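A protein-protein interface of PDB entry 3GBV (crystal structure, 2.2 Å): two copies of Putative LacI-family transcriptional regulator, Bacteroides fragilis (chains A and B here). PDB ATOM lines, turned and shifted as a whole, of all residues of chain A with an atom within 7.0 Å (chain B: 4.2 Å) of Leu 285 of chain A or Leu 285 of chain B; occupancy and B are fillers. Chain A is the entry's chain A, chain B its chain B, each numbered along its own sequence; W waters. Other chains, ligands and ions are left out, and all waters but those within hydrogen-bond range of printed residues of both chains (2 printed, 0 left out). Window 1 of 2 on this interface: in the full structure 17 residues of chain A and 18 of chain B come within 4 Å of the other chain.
Phe 123 of chain A touches Asn 290 of chain B.
CE of Met 127 of chain B touches CE of Met 127 of chain A, at 3.8 Å.
Leu 130 of chain A touches Phe 248 of chain B (CD2 to CZ, 3.8 Å).
CD2 of Leu 285 of chain B touches CD2 of Leu 285 of chain A, at 3.2 Å.
Thr 287 of chain A touches Phe 123 of chain B.
Asn 290 of chain A touches Phe 123 of chain B (CB to CD1, 3.7 Å).
Of the 17 printed residues of chain A, 7 touch a printed residue of chain B.
Hydrophobic or aromatic side chains of chain A within 4 Å of the printed part of chain B: Phe 123, Met 127, Leu 130, Ile 283 and Leu 285.
Printed residues of chain B that touch a printed residue of chain A: Phe 123, Met 127, Phe 248, Ile 283, Leu 285 and Asn 290.
Hydrophobic or aromatic side chains of chain B within 4 Å of the printed part of chain A: Phe 123, Met 127, Phe 248, Ile 283 and Leu 285.
Along chain B the printed residues that touch a printed residue of chain A span positions 123 to 290.
The backbone carbonyl oxygen (O) of Leu 285 of chain A lies close to the side-chain amide oxygen (OD1) of Asn 290 of chain A (3.4 Å).
The side-chain amide nitrogen (ND2) of Asn 290 of chain A sits close to the backbone NH (N) of Thr 287 of chain A (2.7 Å).
The backbone carbonyl oxygen (O) of Leu 285 of chain B sits close to the side-chain amide oxygen (OD1) of Asn 290 of chain B (3.3 Å).
O of Ile 283 of chain A lies close to OD1 of Asn 290 of chain B (3.1 Å).
OD1 of Asn 290 of chain A lies close to O of Ile 283 of chain B (3.1 Å).
Phe 123 of chain A touches Asn 290 of chain B, and with the chains exchanged Asn 290 of chain A touches Phe 123 of chain B.
Met 127 of chain B touches its own counterpart, Met 127 of chain A.
Ile 283 of chain A touches Asn 290 of chain B, and with the chains exchanged Asn 290 of chain A touches Ile 283 of chain B.
Leu 285 of chain A touches its own counterpart, Leu 285 of chain B.
Of the 8 pairs that touch across the chains among the printed residues, 6 have their exchanged pair printed and touching as well.
Water W2 lies within hydrogen-bond range of N of Ile 283 of chain A (2.7 Å) and O of Asn 290 of chain B (2.9 Å).
Water W1 lies within hydrogen-bond range of N of Ile 283 of chain B (2.8 Å), O of Asn 290 of chain A (2.9 Å) and N of Tyr 294 of chain A (3.4 Å).
Of the printed residues of chain B, Leu 285 of chain A touches Leu 285.
Leu 285 of chain B touches just one residue of chain A: Leu 285 (3.2 Å).
Of the printed residues of chain A, Phe 123 of chain B touches Thr 287 and Asn 290.
Printed residues of chain B within 4 Å of Thr 287 of chain A: Phe 123 (3.3 Å).
Printed residues of chain B within 4 Å of Met 127 of chain A: Met 127 (3.8 Å).
The nearest printed residue of chain B that does not touch Leu 285 of chain A is Met 127 of chain B (4.3 Å).
The nearest residue of chain A that does not touch Leu 285 of chain B is Met 127 of chain A (4.3 Å).
The nearest printed residue of chain B that does not touch Ile 283 of chain A is Leu 285 of chain B (5.6 Å).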
ATOM      1  N   PHE A 123      15.821  23.379  31.310  1.00  0.00           N
ATOM      2  CA  PHE A 123      15.176  22.078  31.145  1.00  0.00           C
ATOM      3  C   PHE A 123      15.279  21.255  32.429  1.00  0.00           C
ATOM      4  O   PHE A 123      14.320  20.581  32.827  1.00  0.00           O
ATOM      5  CB  PHE A 123      15.848  21.303  30.000  1.00  0.00           C
ATOM      6  CG  PHE A 123      15.449  19.849  29.921  1.00  0.00           C
ATOM      7  CD1 PHE A 123      14.297  19.456  29.248  1.00  0.00           C
ATOM      8  CD2 PHE A 123      16.238  18.871  30.514  1.00  0.00           C
ATOM      9  CE1 PHE A 123      13.945  18.102  29.163  1.00  0.00           C
ATOM     10  CE2 PHE A 123      15.890  17.517  30.434  1.00  0.00           C
ATOM     11  CZ  PHE A 123      14.744  17.132  29.757  1.00  0.00           C
ATOM     12  N   MET A 127      12.230  19.557  34.817  1.00  0.00           N
ATOM     13  CA  MET A 127      12.184  18.157  35.251  1.00  0.00           C
ATOM     14  C   MET A 127      12.222  17.992  36.766  1.00  0.00           C
ATOM     15  O   MET A 127      11.563  17.106  37.313  1.00  0.00           O
ATOM     16  CB  MET A 127      13.333  17.346  34.629  1.00  0.00           C
ATOM     17  CG  MET A 127      13.349  17.310  33.100  1.00  0.00           C
ATOM     18  SD  MET A 127      11.636  16.672  32.417  1.00  0.00           S
ATOM     19  CE  MET A 127      11.556  14.798  33.108  1.00  0.00           C
ATOM     20  N   LEU A 130       8.847  18.724  38.343  1.00  0.00           N
ATOM     21  CA  LEU A 130       7.835  17.712  38.034  1.00  0.00           C
ATOM     22  C   LEU A 130       7.908  16.722  39.199  1.00  0.00           C
ATOM     23  O   LEU A 130       6.924  16.085  39.573  1.00  0.00           O
ATOM     24  CB  LEU A 130       8.187  16.976  36.731  1.00  0.00           C
ATOM     25  CG  LEU A 130       7.352  15.718  36.420  1.00  0.00           C
ATOM     26  CD1 LEU A 130       5.961  16.139  35.962  1.00  0.00           C
ATOM     27  CD2 LEU A 130       8.029  14.868  35.337  1.00  0.00           C
ATOM     28  N   ILE A 229      18.758  14.642  40.573  1.00  0.00           N
ATOM     29  CA  ILE A 229      18.718  14.808  39.135  1.00  0.00           C
ATOM     30  C   ILE A 229      20.194  15.078  38.872  1.00  0.00           C
ATOM     31  O   ILE A 229      20.802  15.934  39.509  1.00  0.00           O
ATOM     32  CB  ILE A 229      17.872  16.006  38.683  1.00  0.00           C
ATOM     33  CG1 ILE A 229      16.393  15.625  38.725  1.00  0.00           C
ATOM     34  CG2 ILE A 229      18.270  16.425  37.248  1.00  0.00           C
ATOM     35  CD1 ILE A 229      15.493  16.623  38.029  1.00  0.00           C
ATOM     36  N   SER A 247      16.846  10.108  40.090  1.00  0.00           N
ATOM     37  CA  SER A 247      15.588   9.968  39.346  1.00  0.00           C
ATOM     38  C   SER A 247      15.753  10.202  37.852  1.00  0.00           C
ATOM     39  O   SER A 247      15.131   9.526  37.038  1.00  0.00           O
ATOM     40  CB  SER A 247      14.536  10.947  39.876  1.00  0.00           C
ATOM     41  OG  SER A 247      14.296  10.741  41.253  1.00  0.00           O
ATOM     42  N   PHE A 248      16.577  11.178  37.502  1.00  0.00           N
ATOM     43  CA  PHE A 248      16.825  11.488  36.110  1.00  0.00           C
ATOM     44  C   PHE A 248      18.307  11.789  35.921  1.00  0.00           C
ATOM     45  O   PHE A 248      18.980  12.287  36.832  1.00  0.00           O
ATOM     46  CB  PHE A 248      16.037  12.730  35.660  1.00  0.00           C
ATOM     47  CG  PHE A 248      14.538  12.602  35.775  1.00  0.00           C
ATOM     48  CD1 PHE A 248      13.851  11.589  35.113  1.00  0.00           C
ATOM     49  CD2 PHE A 248      13.806  13.532  36.515  1.00  0.00           C
ATOM     50  CE1 PHE A 248      12.462  11.507  35.185  1.00  0.00           C
ATOM     51  CE2 PHE A 248      12.413  13.454  36.592  1.00  0.00           C
ATOM     52  CZ  PHE A 248      11.737  12.441  35.925  1.00  0.00           C
ATOM     53  N   LEU A 249      18.801  11.464  34.732  1.00  0.00           N
ATOM     54  CA  LEU A 249      20.168  11.769  34.346  1.00  0.00           C
ATOM     55  C   LEU A 249      20.033  12.464  32.992  1.00  0.00           C
ATOM     56  O   LEU A 249      19.245  12.046  32.141  1.00  0.00           O
ATOM     57  CB  LEU A 249      21.028  10.505  34.205  1.00  0.00           C
ATOM     58  CG  LEU A 249      21.438   9.791  35.500  1.00  0.00           C
ATOM     59  CD1 LEU A 249      22.200   8.508  35.166  1.00  0.00           C
ATOM     60  CD2 LEU A 249      22.293  10.723  36.356  1.00  0.00           C
ATOM     61  N   ILE A 250      20.782  13.543  32.807  1.00  0.00           N
ATOM     62  CA  ILE A 250      20.759  14.271  31.552  1.00  0.00           C
ATOM     63  C   ILE A 250      22.054  13.954  30.832  1.00  0.00           C
ATOM     64  O   ILE A 250      23.136  14.122  31.387  1.00  0.00           O
ATOM     65  CB  ILE A 250      20.636  15.779  31.798  1.00  0.00           C
ATOM     66  CG1 ILE A 250      19.277  16.064  32.468  1.00  0.00           C
ATOM     67  CG2 ILE A 250      20.806  16.534  30.486  1.00  0.00           C
ATOM     68  CD1 ILE A 250      19.106  17.487  32.996  1.00  0.00           C
ATOM     69  N   ALA A 251      21.943  13.465  29.601  1.00  0.00           N
ATOM     70  CA  ALA A 251      23.121  13.108  28.822  1.00  0.00           C
ATOM     71  C   ALA A 251      23.380  14.116  27.712  1.00  0.00           C
ATOM     72  O   ALA A 251      22.482  14.856  27.308  1.00  0.00           O
ATOM     73  CB  ALA A 251      22.947  11.715  28.237  1.00  0.00           C
ATOM     74  N   ILE A 283      19.927  17.549  24.703  1.00  0.00           N
ATOM     75  CA  ILE A 283      19.685  17.520  26.144  1.00  0.00           C
ATOM     76  C   ILE A 283      18.802  16.283  26.372  1.00  0.00           C
ATOM     77  O   ILE A 283      17.579  16.380  26.490  1.00  0.00           O
ATOM     78  CB  ILE A 283      18.967  18.832  26.566  1.00  0.00           C
ATOM     79  CG1 ILE A 283      19.892  20.025  26.267  1.00  0.00           C
ATOM     80  CG2 ILE A 283      18.572  18.793  28.033  1.00  0.00           C
ATOM     81  CD1 ILE A 283      19.177  21.356  26.233  1.00  0.00           C
ATOM     82  N   ASP A 284      19.438  15.114  26.403  1.00  0.00           N
ATOM     83  CA  ASP A 284      18.723  13.853  26.567  1.00  0.00           C
ATOM     84  C   ASP A 284      18.331  13.505  27.999  1.00  0.00           C
ATOM     85  O   ASP A 284      19.151  13.567  28.920  1.00  0.00           O
ATOM     86  CB  ASP A 284      19.542  12.690  25.989  1.00  0.00           C
ATOM     87  CG  ASP A 284      19.789  12.831  24.491  1.00  0.00           C
ATOM     88  OD1 ASP A 284      18.893  13.344  23.787  1.00  0.00           O
ATOM     89  OD2 ASP A 284      20.876  12.413  24.019  1.00  0.00           O
ATOM     90  N   LEU A 285      17.067  13.133  28.177  1.00  0.00           N
ATOM     91  CA  LEU A 285      16.578  12.745  29.488  1.00  0.00           C
ATOM     92  C   LEU A 285      16.516  11.226  29.626  1.00  0.00           C
ATOM     93  O   LEU A 285      15.894  10.531  28.815  1.00  0.00           O
ATOM     94  CB  LEU A 285      15.191  13.317  29.742  1.00  0.00           C
ATOM     95  CG  LEU A 285      14.777  12.950  31.158  1.00  0.00           C
ATOM     96  CD1 LEU A 285      15.291  14.021  32.122  1.00  0.00           C
ATOM     97  CD2 LEU A 285      13.280  12.798  31.220  1.00  0.00           C
ATOM     98  N   LEU A 286      17.166  10.708  30.655  1.00  0.00           N
ATOM     99  CA  LEU A 286      17.158   9.275  30.872  1.00  0.00           C
ATOM    100  C   LEU A 286      16.584   8.903  32.225  1.00  0.00           C
ATOM    101  O   LEU A 286      16.752   9.621  33.218  1.00  0.00           O
ATOM    102  CB  LEU A 286      18.571   8.719  30.690  1.00  0.00           C
ATOM    103  CG  LEU A 286      18.921   8.878  29.204  1.00  0.00           C
ATOM    104  CD1 LEU A 286      20.373   9.231  29.024  1.00  0.00           C
ATOM    105  CD2 LEU A 286      18.551   7.613  28.460  1.00  0.00           C
ATOM    106  N   THR A 287      15.855   7.794  32.242  1.00  0.00           N
ATOM    107  CA  THR A 287      15.256   7.290  33.471  1.00  0.00           C
ATOM    108  C   THR A 287      15.603   5.812  33.549  1.00  0.00           C
ATOM    109  O   THR A 287      16.158   5.245  32.611  1.00  0.00           O
ATOM    110  CB  THR A 287      13.716   7.427  33.470  1.00  0.00           C
ATOM    111  OG1 THR A 287      13.146   6.476  32.565  1.00  0.00           O
ATOM    112  CG2 THR A 287      13.308   8.810  33.041  1.00  0.00           C
ATOM    113  N   ASN A 290      14.250   3.730  30.551  1.00  0.00           N
ATOM    114  CA  ASN A 290      14.681   3.837  29.160  1.00  0.00           C
ATOM    115  C   ASN A 290      16.199   3.832  28.990  1.00  0.00           C
ATOM    116  O   ASN A 290      16.707   3.793  27.865  1.00  0.00           O
ATOM    117  CB  ASN A 290      14.079   5.086  28.489  1.00  0.00           C
ATOM    118  CG  ASN A 290      14.756   6.390  28.914  1.00  0.00           C
ATOM    119  OD1 ASN A 290      14.602   7.420  28.241  1.00  0.00           O
ATOM    120  ND2 ASN A 290      15.490   6.361  30.026  1.00  0.00           N
ATOM    121  N   ILE A 291      16.918   3.838  30.111  1.00  0.00           N
ATOM    122  CA  ILE A 291      18.369   3.859  30.065  1.00  0.00           C
ATOM    123  C   ILE A 291      18.988   2.716  29.268  1.00  0.00           C
ATOM    124  O   ILE A 291      19.976   2.930  28.573  1.00  0.00           O
ATOM    125  CB  ILE A 291      19.002   3.875  31.492  1.00  0.00           C
ATOM    126  CG1 ILE A 291      20.516   4.056  31.390  1.00  0.00           C
ATOM    127  CG2 ILE A 291      18.750   2.567  32.208  1.00  0.00           C
ATOM    128  CD1 ILE A 291      20.946   5.352  30.742  1.00  0.00           C
ATOM    129  N   TYR A 294      19.032   3.388  25.312  1.00  0.00           N
ATOM    130  CA  TYR A 294      19.691   4.605  24.833  1.00  0.00           C
ATOM    131  C   TYR A 294      21.062   4.237  24.279  1.00  0.00           C
ATOM    132  O   TYR A 294      21.752   3.388  24.840  1.00  0.00           O
ATOM    133  CB  TYR A 294      19.869   5.587  25.995  1.00  0.00           C
ATOM    134  CG  TYR A 294      20.566   6.883  25.653  1.00  0.00           C
ATOM    135  CD1 TYR A 294      19.855   7.974  25.145  1.00  0.00           C
ATOM    136  CD2 TYR A 294      21.929   7.038  25.874  1.00  0.00           C
ATOM    137  CE1 TYR A 294      20.487   9.184  24.875  1.00  0.00           C
ATOM    138  CE2 TYR A 294      22.569   8.240  25.605  1.00  0.00           C
ATOM    139  CZ  TYR A 294      21.844   9.305  25.109  1.00  0.00           C
ATOM    140  OH  TYR A 294      22.471  10.489  24.840  1.00  0.00           O
ATOM    141  N   PHE B 123       7.575   2.672  30.460  1.00  0.00           N
ATOM    142  CA  PHE B 123       8.195   3.981  30.580  1.00  0.00           C
ATOM    143  C   PHE B 123       7.130   5.083  30.544  1.00  0.00           C
ATOM    144  O   PHE B 123       7.140   5.986  31.382  1.00  0.00           O
ATOM    145  CB  PHE B 123       9.189   4.201  29.434  1.00  0.00           C
ATOM    146  CG  PHE B 123       9.702   5.614  29.339  1.00  0.00           C
ATOM    147  CD1 PHE B 123      10.820   6.016  30.054  1.00  0.00           C
ATOM    148  CD2 PHE B 123       9.046   6.553  28.546  1.00  0.00           C
ATOM    149  CE1 PHE B 123      11.275   7.330  29.979  1.00  0.00           C
ATOM    150  CE2 PHE B 123       9.497   7.865  28.468  1.00  0.00           C
ATOM    151  CZ  PHE B 123      10.609   8.253  29.179  1.00  0.00           C
ATOM    152  N   MET B 127       6.156   8.038  33.395  1.00  0.00           N
ATOM    153  CA  MET B 127       6.150   9.474  33.127  1.00  0.00           C
ATOM    154  C   MET B 127       4.767  10.059  33.384  1.00  0.00           C
ATOM    155  O   MET B 127       4.655  11.150  33.917  1.00  0.00           O
ATOM    156  CB  MET B 127       6.573   9.769  31.678  1.00  0.00           C
ATOM    157  CG  MET B 127       7.959   9.264  31.305  1.00  0.00           C
ATOM    158  SD  MET B 127       9.287  10.119  32.511  1.00  0.00           S
ATOM    159  CE  MET B 127       9.105  12.049  32.080  1.00  0.00           C
ATOM    160  N   PHE B 248       4.428  15.616  27.208  1.00  0.00           N
ATOM    161  CA  PHE B 248       5.596  14.859  26.744  1.00  0.00           C
ATOM    162  C   PHE B 248       5.284  14.116  25.447  1.00  0.00           C
ATOM    163  O   PHE B 248       4.137  13.726  25.195  1.00  0.00           O
ATOM    164  CB  PHE B 248       6.007  13.785  27.755  1.00  0.00           C
ATOM    165  CG  PHE B 248       6.360  14.304  29.115  1.00  0.00           C
ATOM    166  CD1 PHE B 248       7.439  15.159  29.296  1.00  0.00           C
ATOM    167  CD2 PHE B 248       5.639  13.887  30.229  1.00  0.00           C
ATOM    168  CE1 PHE B 248       7.804  15.589  30.570  1.00  0.00           C
ATOM    169  CE2 PHE B 248       5.992  14.310  31.509  1.00  0.00           C
ATOM    170  CZ  PHE B 248       7.081  15.165  31.681  1.00  0.00           C
ATOM    171  N   LEU B 249       6.309  13.922  24.624  1.00  0.00           N
ATOM    172  CA  LEU B 249       6.159  13.138  23.398  1.00  0.00           C
ATOM    173  C   LEU B 249       7.256  12.102  23.467  1.00  0.00           C
ATOM    174  O   LEU B 249       8.359  12.407  23.908  1.00  0.00           O
ATOM    175  CB  LEU B 249       6.330  13.989  22.140  1.00  0.00           C
ATOM    176  CG  LEU B 249       5.170  14.929  21.789  1.00  0.00           C
ATOM    177  CD1 LEU B 249       5.564  15.839  20.612  1.00  0.00           C
ATOM    178  CD2 LEU B 249       3.941  14.106  21.434  1.00  0.00           C
ATOM    179  N   ILE B 283      13.836   5.029  23.476  1.00  0.00           N
ATOM    180  CA  ILE B 283      12.550   5.527  23.932  1.00  0.00           C
ATOM    181  C   ILE B 283      12.893   6.956  24.360  1.00  0.00           C
ATOM    182  O   ILE B 283      13.172   7.214  25.533  1.00  0.00           O
ATOM    183  CB  ILE B 283      12.048   4.679  25.142  1.00  0.00           C
ATOM    184  CG1 ILE B 283      11.871   3.218  24.700  1.00  0.00           C
ATOM    185  CG2 ILE B 283      10.744   5.245  25.707  1.00  0.00           C
ATOM    186  CD1 ILE B 283      11.736   2.209  25.858  1.00  0.00           C
ATOM    187  N   ASP B 284      12.905   7.870  23.390  1.00  0.00           N
ATOM    188  CA  ASP B 284      13.268   9.260  23.643  1.00  0.00           C
ATOM    189  C   ASP B 284      12.137  10.129  24.162  1.00  0.00           C
ATOM    190  O   ASP B 284      11.051  10.185  23.572  1.00  0.00           O
ATOM    191  CB  ASP B 284      13.859   9.912  22.385  1.00  0.00           C
ATOM    192  CG  ASP B 284      15.121   9.209  21.889  1.00  0.00           C
ATOM    193  OD1 ASP B 284      15.868   8.620  22.708  1.00  0.00           O
ATOM    194  OD2 ASP B 284      15.372   9.258  20.670  1.00  0.00           O
ATOM    195  N   LEU B 285      12.418  10.822  25.263  1.00  0.00           N
ATOM    196  CA  LEU B 285      11.443  11.699  25.883  1.00  0.00           C
ATOM    197  C   LEU B 285      11.703  13.138  25.502  1.00  0.00           C
ATOM    198  O   LEU B 285      12.790  13.670  25.730  1.00  0.00           O
ATOM    199  CB  LEU B 285      11.476  11.580  27.406  1.00  0.00           C
ATOM    200  CG  LEU B 285      10.336  12.409  28.013  1.00  0.00           C
ATOM    201  CD1 LEU B 285       9.144  11.516  28.276  1.00  0.00           C
ATOM    202  CD2 LEU B 285      10.799  13.103  29.275  1.00  0.00           C
ATOM    203  N   LEU B 286      10.691  13.772  24.927  1.00  0.00           N
ATOM    204  CA  LEU B 286      10.808  15.159  24.522  1.00  0.00           C
ATOM    205  C   LEU B 286       9.841  16.057  25.277  1.00  0.00           C
ATOM    206  O   LEU B 286       8.702  15.670  25.563  1.00  0.00           O
ATOM    207  CB  LEU B 286      10.550  15.298  23.012  1.00  0.00           C
ATOM    208  CG  LEU B 286      11.588  14.723  22.032  1.00  0.00           C
ATOM    209  CD1 LEU B 286      12.956  15.280  22.398  1.00  0.00           C
ATOM    210  CD2 LEU B 286      11.614  13.183  22.074  1.00  0.00           C
ATOM    211  N   ASN B 290      13.436  20.703  25.556  1.00  0.00           N
ATOM    212  CA  ASN B 290      14.607  20.036  24.985  1.00  0.00           C
ATOM    213  C   ASN B 290      14.412  19.609  23.536  1.00  0.00           C
ATOM    214  O   ASN B 290      15.364  19.192  22.875  1.00  0.00           O
ATOM    215  CB  ASN B 290      15.041  18.833  25.848  1.00  0.00           C
ATOM    216  CG  ASN B 290      14.129  17.627  25.701  1.00  0.00           C
ATOM    217  OD1 ASN B 290      14.535  16.502  25.998  1.00  0.00           O
ATOM    218  ND2 ASN B 290      12.903  17.851  25.256  1.00  0.00           N
HETATM  219  O   HOH W   1      15.992   4.892  25.328  1.00  0.00           O
HETATM  220  O   HOH W   2      17.737  17.583  23.153  1.00  0.00           O
